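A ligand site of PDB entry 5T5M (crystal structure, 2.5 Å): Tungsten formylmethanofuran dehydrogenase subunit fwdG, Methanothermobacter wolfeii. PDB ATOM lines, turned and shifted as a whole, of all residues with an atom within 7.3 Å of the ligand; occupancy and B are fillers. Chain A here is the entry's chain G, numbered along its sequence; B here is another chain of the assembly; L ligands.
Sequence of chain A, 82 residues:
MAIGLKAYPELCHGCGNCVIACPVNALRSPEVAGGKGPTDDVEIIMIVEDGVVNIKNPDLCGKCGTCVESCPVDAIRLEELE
FE3 of the ligand is bound by SG of Cys 71, 2.4 Å away.
The side-chain sulfur (SG) of Cys 18 binds an iron atom (FE1) of the ligand.
S3 of the ligand sits close to N of Cys 15, 3.7 Å away.
N of Gly 16 lies close to S3 of the ligand (3.7 Å).
SG of Cys 12 is bound to FE4 of the ligand (2.5 Å).
N of His 13 sits close to S1 of the ligand (3.7 Å).
The side-chain sulfur (SG) of Cys 15 is bound to an iron atom (FE2) of the ligand, at 2.5 Å.
SG of Cys 71 lies close to N of Val 73.
The side-chain sulfur of Cys 71 sits close to the backbone NH of Asp 74 (3.3 Å).
The backbone carbonyl oxygen (O) of Met 154 of chain B lies within hydrogen-bond range of a ring nitrogen (ND1) of His 13.
The side-chain sulfur of Cys 15 sits close to the side-chain amide oxygen of Asn 17, at 3.3 Å.
N of Gly 14 lies close to SG of Cys 12, at 3.0 Å.
N of Ala 75 sits close to SG of Cys 71 (3.4 Å).
The backbone carbonyl oxygen (O) of Ala 75 lies within hydrogen-bond range of the backbone NH (N) of Tyr 8, 2.8 Å away.
The backbone NH of Val 53 sits close to the side-chain sulfur of Cys 12.
N of Gly 14 touches FE4 of the ligand, 3.8 Å away.
Val 73 touches the ligand.
Ala 75 touches the ligand.
Ile 76 touches the ligand (CG2 to S2, 3.8 Å).
Hydrophobic or aromatic side chains that line the ligand: Val 73, Ala 75 and Ile 76.
Of the 29 residues printed, 10 come within 4 Å of the ligand.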
ATOM      1  N   ALA A   7     -26.054  21.523 -25.552  1.00  0.00           N
ATOM      2  CA  ALA A   7     -24.615  21.627 -25.415  1.00  0.00           C
ATOM      3  C   ALA A   7     -24.213  22.219 -24.065  1.00  0.00           C
ATOM      4  O   ALA A   7     -24.972  22.976 -23.441  1.00  0.00           O
ATOM      5  CB  ALA A   7     -24.020  22.486 -26.538  1.00  0.00           C
ATOM      6  N   TYR A   8     -23.011  21.857 -23.635  1.00  0.00           N
ATOM      7  CA  TYR A   8     -22.376  22.409 -22.436  1.00  0.00           C
ATOM      8  C   TYR A   8     -20.995  22.897 -22.835  1.00  0.00           C
ATOM      9  O   TYR A   8     -19.981  22.277 -22.516  1.00  0.00           O
ATOM     10  CB  TYR A   8     -22.296  21.359 -21.324  1.00  0.00           C
ATOM     11  CG  TYR A   8     -23.635  20.969 -20.770  1.00  0.00           C
ATOM     12  CD1 TYR A   8     -24.491  20.159 -21.503  1.00  0.00           C
ATOM     13  CD2 TYR A   8     -24.044  21.407 -19.515  1.00  0.00           C
ATOM     14  CE1 TYR A   8     -25.729  19.793 -21.013  1.00  0.00           C
ATOM     15  CE2 TYR A   8     -25.280  21.042 -19.012  1.00  0.00           C
ATOM     16  CZ  TYR A   8     -26.118  20.239 -19.755  1.00  0.00           C
ATOM     17  OH  TYR A   8     -27.350  19.868 -19.258  1.00  0.00           O
ATOM     18  N   PRO A   9     -20.925  24.015 -23.556  1.00  0.00           N
ATOM     19  CA  PRO A   9     -19.642  24.430 -24.136  1.00  0.00           C
ATOM     20  C   PRO A   9     -18.542  24.618 -23.117  1.00  0.00           C
ATOM     21  O   PRO A   9     -17.359  24.574 -23.491  1.00  0.00           O
ATOM     22  CB  PRO A   9     -19.986  25.755 -24.842  1.00  0.00           C
ATOM     23  CG  PRO A   9     -21.186  26.247 -24.149  1.00  0.00           C
ATOM     24  CD  PRO A   9     -21.965  25.043 -23.758  1.00  0.00           C
ATOM     25  N   LEU A  11     -17.741  22.546 -20.842  1.00  0.00           N
ATOM     26  CA  LEU A  11     -17.121  21.252 -20.601  1.00  0.00           C
ATOM     27  C   LEU A  11     -16.424  20.713 -21.834  1.00  0.00           C
ATOM     28  O   LEU A  11     -15.722  19.700 -21.738  1.00  0.00           O
ATOM     29  CB  LEU A  11     -18.180  20.236 -20.159  1.00  0.00           C
ATOM     30  CG  LEU A  11     -18.920  20.565 -18.867  1.00  0.00           C
ATOM     31  CD1 LEU A  11     -19.941  19.474 -18.556  1.00  0.00           C
ATOM     32  CD2 LEU A  11     -17.925  20.736 -17.719  1.00  0.00           C
ATOM     33  N   CYS A  12     -16.589  21.380 -22.974  1.00  0.00           N
ATOM     34  CA  CYS A  12     -16.244  20.836 -24.272  1.00  0.00           C
ATOM     35  C   CYS A  12     -14.789  21.088 -24.622  1.00  0.00           C
ATOM     36  O   CYS A  12     -14.240  22.162 -24.374  1.00  0.00           O
ATOM     37  CB  CYS A  12     -17.165  21.469 -25.335  1.00  0.00           C
ATOM     38  SG  CYS A  12     -16.588  21.460 -27.036  1.00  0.00           S
ATOM     39  N   HIS A  13     -14.141  20.069 -25.208  1.00  0.00           N
ATOM     40  CA  HIS A  13     -12.773  20.192 -25.668  1.00  0.00           C
ATOM     41  C   HIS A  13     -12.693  20.664 -27.106  1.00  0.00           C
ATOM     42  O   HIS A  13     -11.594  20.991 -27.581  1.00  0.00           O
ATOM     43  CB  HIS A  13     -12.038  18.846 -25.548  1.00  0.00           C
ATOM     44  CG  HIS A  13     -11.889  18.352 -24.148  1.00  0.00           C
ATOM     45  ND1 HIS A  13     -10.871  17.516 -23.767  1.00  0.00           N
ATOM     46  CD2 HIS A  13     -12.633  18.578 -23.044  1.00  0.00           C
ATOM     47  CE1 HIS A  13     -10.984  17.240 -22.478  1.00  0.00           C
ATOM     48  NE2 HIS A  13     -12.052  17.876 -22.012  1.00  0.00           N
ATOM     49  N   GLY A  14     -13.822  20.725 -27.808  1.00  0.00           N
ATOM     50  CA  GLY A  14     -13.802  21.029 -29.218  1.00  0.00           C
ATOM     51  C   GLY A  14     -13.131  19.932 -30.012  1.00  0.00           C
ATOM     52  O   GLY A  14     -12.566  20.202 -31.079  1.00  0.00           O
ATOM     53  N   CYS A  15     -13.188  18.697 -29.514  1.00  0.00           N
ATOM     54  CA  CYS A  15     -12.446  17.602 -30.109  1.00  0.00           C
ATOM     55  C   CYS A  15     -13.051  17.122 -31.428  1.00  0.00           C
ATOM     56  O   CYS A  15     -12.348  16.530 -32.245  1.00  0.00           O
ATOM     57  CB  CYS A  15     -12.361  16.459 -29.101  1.00  0.00           C
ATOM     58  SG  CYS A  15     -13.774  15.322 -29.133  1.00  0.00           S
ATOM     59  N   GLY A  16     -14.347  17.356 -31.638  1.00  0.00           N
ATOM     60  CA  GLY A  16     -14.973  17.049 -32.904  1.00  0.00           C
ATOM     61  C   GLY A  16     -15.564  15.662 -33.015  1.00  0.00           C
ATOM     62  O   GLY A  16     -16.185  15.365 -34.039  1.00  0.00           O
ATOM     63  N   ASN A  17     -15.386  14.795 -32.009  1.00  0.00           N
ATOM     64  CA  ASN A  17     -15.953  13.450 -32.084  1.00  0.00           C
ATOM     65  C   ASN A  17     -17.419  13.516 -32.505  1.00  0.00           C
ATOM     66  O   ASN A  17     -17.836  12.832 -33.447  1.00  0.00           O
ATOM     67  CB  ASN A  17     -15.818  12.731 -30.741  1.00  0.00           C
ATOM     68  CG  ASN A  17     -14.381  12.370 -30.409  1.00  0.00           C
ATOM     69  OD1 ASN A  17     -13.458  12.723 -31.141  1.00  0.00           O
ATOM     70  ND2 ASN A  17     -14.187  11.662 -29.303  1.00  0.00           N
ATOM     71  N   CYS A  18     -18.196  14.343 -31.808  1.00  0.00           N
ATOM     72  CA  CYS A  18     -19.632  14.393 -32.037  1.00  0.00           C
ATOM     73  C   CYS A  18     -19.946  14.804 -33.472  1.00  0.00           C
ATOM     74  O   CYS A  18     -20.795  14.184 -34.136  1.00  0.00           O
ATOM     75  CB  CYS A  18     -20.267  15.365 -31.038  1.00  0.00           C
ATOM     76  SG  CYS A  18     -19.891  17.083 -31.345  1.00  0.00           S
ATOM     77  N   VAL A  19     -19.275  15.840 -33.980  1.00  0.00           N
ATOM     78  CA  VAL A  19     -19.544  16.314 -35.327  1.00  0.00           C
ATOM     79  C   VAL A  19     -19.337  15.192 -36.337  1.00  0.00           C
ATOM     80  O   VAL A  19     -20.121  15.035 -37.289  1.00  0.00           O
ATOM     81  CB  VAL A  19     -18.668  17.530 -35.659  1.00  0.00           C
ATOM     82  CG1 VAL A  19     -18.884  17.953 -37.093  1.00  0.00           C
ATOM     83  CG2 VAL A  19     -18.967  18.681 -34.699  1.00  0.00           C
ATOM     84  N   MET A  46     -24.443  20.680 -35.968  1.00  0.00           N
ATOM     85  CA  MET A  46     -23.537  21.423 -35.103  1.00  0.00           C
ATOM     86  C   MET A  46     -22.135  21.326 -35.683  1.00  0.00           C
ATOM     87  O   MET A  46     -21.843  20.485 -36.530  1.00  0.00           O
ATOM     88  CB  MET A  46     -23.560  20.887 -33.664  1.00  0.00           C
ATOM     89  CG  MET A  46     -22.943  19.513 -33.456  1.00  0.00           C
ATOM     90  SD  MET A  46     -23.990  18.171 -34.072  1.00  0.00           S
ATOM     91  CE  MET A  46     -23.765  16.960 -32.778  1.00  0.00           C
ATOM     92  N   ILE A  47     -21.298  22.255 -35.228  1.00  0.00           N
ATOM     93  CA  ILE A  47     -19.877  22.296 -35.540  1.00  0.00           C
ATOM     94  C   ILE A  47     -19.142  22.653 -34.257  1.00  0.00           C
ATOM     95  O   ILE A  47     -19.755  22.940 -33.232  1.00  0.00           O
ATOM     96  CB  ILE A  47     -19.533  23.338 -36.621  1.00  0.00           C
ATOM     97  CG1 ILE A  47     -20.159  24.679 -36.221  1.00  0.00           C
ATOM     98  CG2 ILE A  47     -19.958  22.859 -37.983  1.00  0.00           C
ATOM     99  CD1 ILE A  47     -19.849  25.808 -37.165  1.00  0.00           C
ATOM    100  N   VAL A  48     -17.820  22.647 -34.351  1.00  0.00           N
ATOM    101  CA  VAL A  48     -16.964  23.280 -33.359  1.00  0.00           C
ATOM    102  C   VAL A  48     -16.691  24.700 -33.855  1.00  0.00           C
ATOM    103  O   VAL A  48     -16.113  24.877 -34.933  1.00  0.00           O
ATOM    104  CB  VAL A  48     -15.664  22.496 -33.153  1.00  0.00           C
ATOM    105  CG1 VAL A  48     -14.744  23.206 -32.178  1.00  0.00           C
ATOM    106  CG2 VAL A  48     -15.974  21.071 -32.660  1.00  0.00           C
ATOM    107  N   GLY A  51     -13.732  27.071 -30.783  1.00  0.00           N
ATOM    108  CA  GLY A  51     -13.150  26.070 -29.908  1.00  0.00           C
ATOM    109  C   GLY A  51     -14.140  25.189 -29.167  1.00  0.00           C
ATOM    110  O   GLY A  51     -13.706  24.348 -28.374  1.00  0.00           O
ATOM    111  N   VAL A  52     -15.440  25.352 -29.375  1.00  0.00           N
ATOM    112  CA  VAL A  52     -16.422  24.564 -28.654  1.00  0.00           C
ATOM    113  C   VAL A  52     -17.566  24.176 -29.579  1.00  0.00           C
ATOM    114  O   VAL A  52     -17.848  24.845 -30.569  1.00  0.00           O
ATOM    115  CB  VAL A  52     -16.987  25.317 -27.435  1.00  0.00           C
ATOM    116  CG1 VAL A  52     -15.940  25.429 -26.351  1.00  0.00           C
ATOM    117  CG2 VAL A  52     -17.459  26.703 -27.862  1.00  0.00           C
ATOM    118  N   VAL A  53     -18.226  23.071 -29.236  1.00  0.00           N
ATOM    119  CA  VAL A  53     -19.369  22.601 -30.000  1.00  0.00           C
ATOM    120  C   VAL A  53     -20.466  23.660 -29.969  1.00  0.00           C
ATOM    121  O   VAL A  53     -20.743  24.260 -28.929  1.00  0.00           O
ATOM    122  CB  VAL A  53     -19.872  21.270 -29.439  1.00  0.00           C
ATOM    123  CG1 VAL A  53     -20.345  21.434 -27.992  1.00  0.00           C
ATOM    124  CG2 VAL A  53     -20.978  20.690 -30.300  1.00  0.00           C
ATOM    125  N   CYS A  67     -23.878  11.027 -30.970  1.00  0.00           N
ATOM    126  CA  CYS A  67     -22.956  12.071 -30.525  1.00  0.00           C
ATOM    127  C   CYS A  67     -22.746  12.006 -29.021  1.00  0.00           C
ATOM    128  O   CYS A  67     -21.619  12.179 -28.541  1.00  0.00           O
ATOM    129  CB  CYS A  67     -23.513  13.439 -30.911  1.00  0.00           C
ATOM    130  SG  CYS A  67     -24.916  14.021 -29.919  1.00  0.00           S
ATOM    131  N   VAL A  68     -23.815  11.731 -28.268  1.00  0.00           N
ATOM    132  CA  VAL A  68     -23.724  11.682 -26.802  1.00  0.00           C
ATOM    133  C   VAL A  68     -22.756  10.592 -26.383  1.00  0.00           C
ATOM    134  O   VAL A  68     -21.929  10.796 -25.478  1.00  0.00           O
ATOM    135  CB  VAL A  68     -25.121  11.479 -26.186  1.00  0.00           C
ATOM    136  CG1 VAL A  68     -25.043  10.997 -24.750  1.00  0.00           C
ATOM    137  CG2 VAL A  68     -25.883  12.753 -26.228  1.00  0.00           C
ATOM    138  N   SER A  70     -20.294   9.383 -27.972  1.00  0.00           N
ATOM    139  CA  SER A  70     -18.950   9.598 -28.469  1.00  0.00           C
ATOM    140  C   SER A  70     -18.231  10.703 -27.714  1.00  0.00           C
ATOM    141  O   SER A  70     -17.058  10.968 -27.990  1.00  0.00           O
ATOM    142  CB  SER A  70     -18.996   9.954 -29.964  1.00  0.00           C
ATOM    143  OG  SER A  70     -19.486  11.272 -30.137  1.00  0.00           O
ATOM    144  N   CYS A  71     -18.902  11.356 -26.757  1.00  0.00           N
ATOM    145  CA  CYS A  71     -18.281  12.374 -25.937  1.00  0.00           C
ATOM    146  C   CYS A  71     -17.990  11.825 -24.554  1.00  0.00           C
ATOM    147  O   CYS A  71     -18.913  11.357 -23.866  1.00  0.00           O
ATOM    148  CB  CYS A  71     -19.178  13.596 -25.821  1.00  0.00           C
ATOM    149  SG  CYS A  71     -18.653  14.680 -24.504  1.00  0.00           S
ATOM    150  N   PRO A  72     -16.740  11.890 -24.082  1.00  0.00           N
ATOM    151  CA  PRO A  72     -16.406  11.369 -22.757  1.00  0.00           C
ATOM    152  C   PRO A  72     -16.585  12.357 -21.612  1.00  0.00           C
ATOM    153  O   PRO A  72     -16.456  11.944 -20.456  1.00  0.00           O
ATOM    154  CB  PRO A  72     -14.924  11.001 -22.918  1.00  0.00           C
ATOM    155  CG  PRO A  72     -14.398  12.012 -23.865  1.00  0.00           C
ATOM    156  CD  PRO A  72     -15.541  12.350 -24.794  1.00  0.00           C
ATOM    157  N   VAL A  73     -16.877  13.623 -21.901  1.00  0.00           N
ATOM    158  CA  VAL A  73     -16.893  14.660 -20.867  1.00  0.00           C
ATOM    159  C   VAL A  73     -18.282  15.284 -20.720  1.00  0.00           C
ATOM    160  O   VAL A  73     -18.417  16.367 -20.144  1.00  0.00           O
ATOM    161  CB  VAL A  73     -15.829  15.742 -21.146  1.00  0.00           C
ATOM    162  CG1 VAL A  73     -14.429  15.123 -21.043  1.00  0.00           C
ATOM    163  CG2 VAL A  73     -16.070  16.393 -22.505  1.00  0.00           C
ATOM    164  N   ASP A  74     -19.307  14.622 -21.244  1.00  0.00           N
ATOM    165  CA  ASP A  74     -20.702  15.014 -21.025  1.00  0.00           C
ATOM    166  C   ASP A  74     -20.945  16.464 -21.450  1.00  0.00           C
ATOM    167  O   ASP A  74     -21.756  17.182 -20.851  1.00  0.00           O
ATOM    168  CB  ASP A  74     -21.090  14.797 -19.569  1.00  0.00           C
ATOM    169  CG  ASP A  74     -20.993  13.338 -19.161  1.00  0.00           C
ATOM    170  OD1 ASP A  74     -21.062  12.474 -20.064  1.00  0.00           O
ATOM    171  OD2 ASP A  74     -20.819  13.053 -17.962  1.00  0.00           O
ATOM    172  N   ALA A  75     -20.261  16.890 -22.514  1.00  0.00           N
ATOM    173  CA  ALA A  75     -20.406  18.237 -23.039  1.00  0.00           C
ATOM    174  C   ALA A  75     -21.527  18.345 -24.056  1.00  0.00           C
ATOM    175  O   ALA A  75     -21.828  19.456 -24.519  1.00  0.00           O
ATOM    176  CB  ALA A  75     -19.091  18.689 -23.691  1.00  0.00           C
ATOM    177  N   ILE A  76     -22.166  17.234 -24.425  1.00  0.00           N
ATOM    178  CA  ILE A  76     -23.334  17.265 -25.298  1.00  0.00           C
ATOM    179  C   ILE A  76     -24.274  16.165 -24.845  1.00  0.00           C
ATOM    180  O   ILE A  76     -23.839  15.028 -24.617  1.00  0.00           O
ATOM    181  CB  ILE A  76     -22.937  17.118 -26.775  1.00  0.00           C
ATOM    182  CG1 ILE A  76     -24.183  17.126 -27.658  1.00  0.00           C
ATOM    183  CG2 ILE A  76     -22.102  15.847 -26.999  1.00  0.00           C
ATOM    184  CD1 ILE A  76     -23.877  17.392 -29.103  1.00  0.00           C
ATOM    185  N   MET B 154      -7.439  13.048 -26.136  1.00  0.00           N
ATOM    186  CA  MET B 154      -8.552  13.955 -25.820  1.00  0.00           C
ATOM    187  C   MET B 154      -8.061  15.262 -25.201  1.00  0.00           C
ATOM    188  O   MET B 154      -8.714  16.299 -25.348  1.00  0.00           O
ATOM    189  CB  MET B 154      -9.538  13.272 -24.875  1.00  0.00           C
ATOM    190  CG  MET B 154     -10.470  12.271 -25.554  1.00  0.00           C
ATOM    191  SD  MET B 154     -11.541  13.022 -26.808  1.00  0.00           S
ATOM    192  CE  MET B 154     -12.326  14.314 -25.861  1.00  0.00           C
ATOM    193  N   PRO B 158      -6.515  16.995 -29.425  1.00  0.00           N
ATOM    194  CA  PRO B 158      -7.961  16.815 -29.236  1.00  0.00           C
ATOM    195  C   PRO B 158      -8.703  16.299 -30.456  1.00  0.00           C
ATOM    196  O   PRO B 158      -9.631  15.491 -30.298  1.00  0.00           O
ATOM    197  CB  PRO B 158      -8.423  18.209 -28.804  1.00  0.00           C
ATOM    198  CG  PRO B 158      -7.188  18.788 -28.101  1.00  0.00           C
ATOM    199  CD  PRO B 158      -6.058  18.315 -28.968  1.00  0.00           C
HETATM  200 FE1  LIG L   1     -18.435  17.156 -29.277  1.00  0.00          FE
HETATM  201 FE2  LIG L   1     -15.684  16.711 -28.248  1.00  0.00          FE
HETATM  202 FE3  LIG L   1     -17.922  16.223 -26.215  1.00  0.00          FE
HETATM  203 FE4  LIG L   1     -17.170  19.002 -27.207  1.00  0.00          FE
HETATM  204  S1  LIG L   1     -16.258  17.316 -26.392  1.00  0.00           S
HETATM  205  S2  LIG L   1     -18.790  17.741 -27.380  1.00  0.00           S
HETATM  206  S3  LIG L   1     -16.820  18.279 -29.073  1.00  0.00           S
HETATM  207  S4  LIG L   1     -17.405  15.718 -28.105  1.00  0.00           S
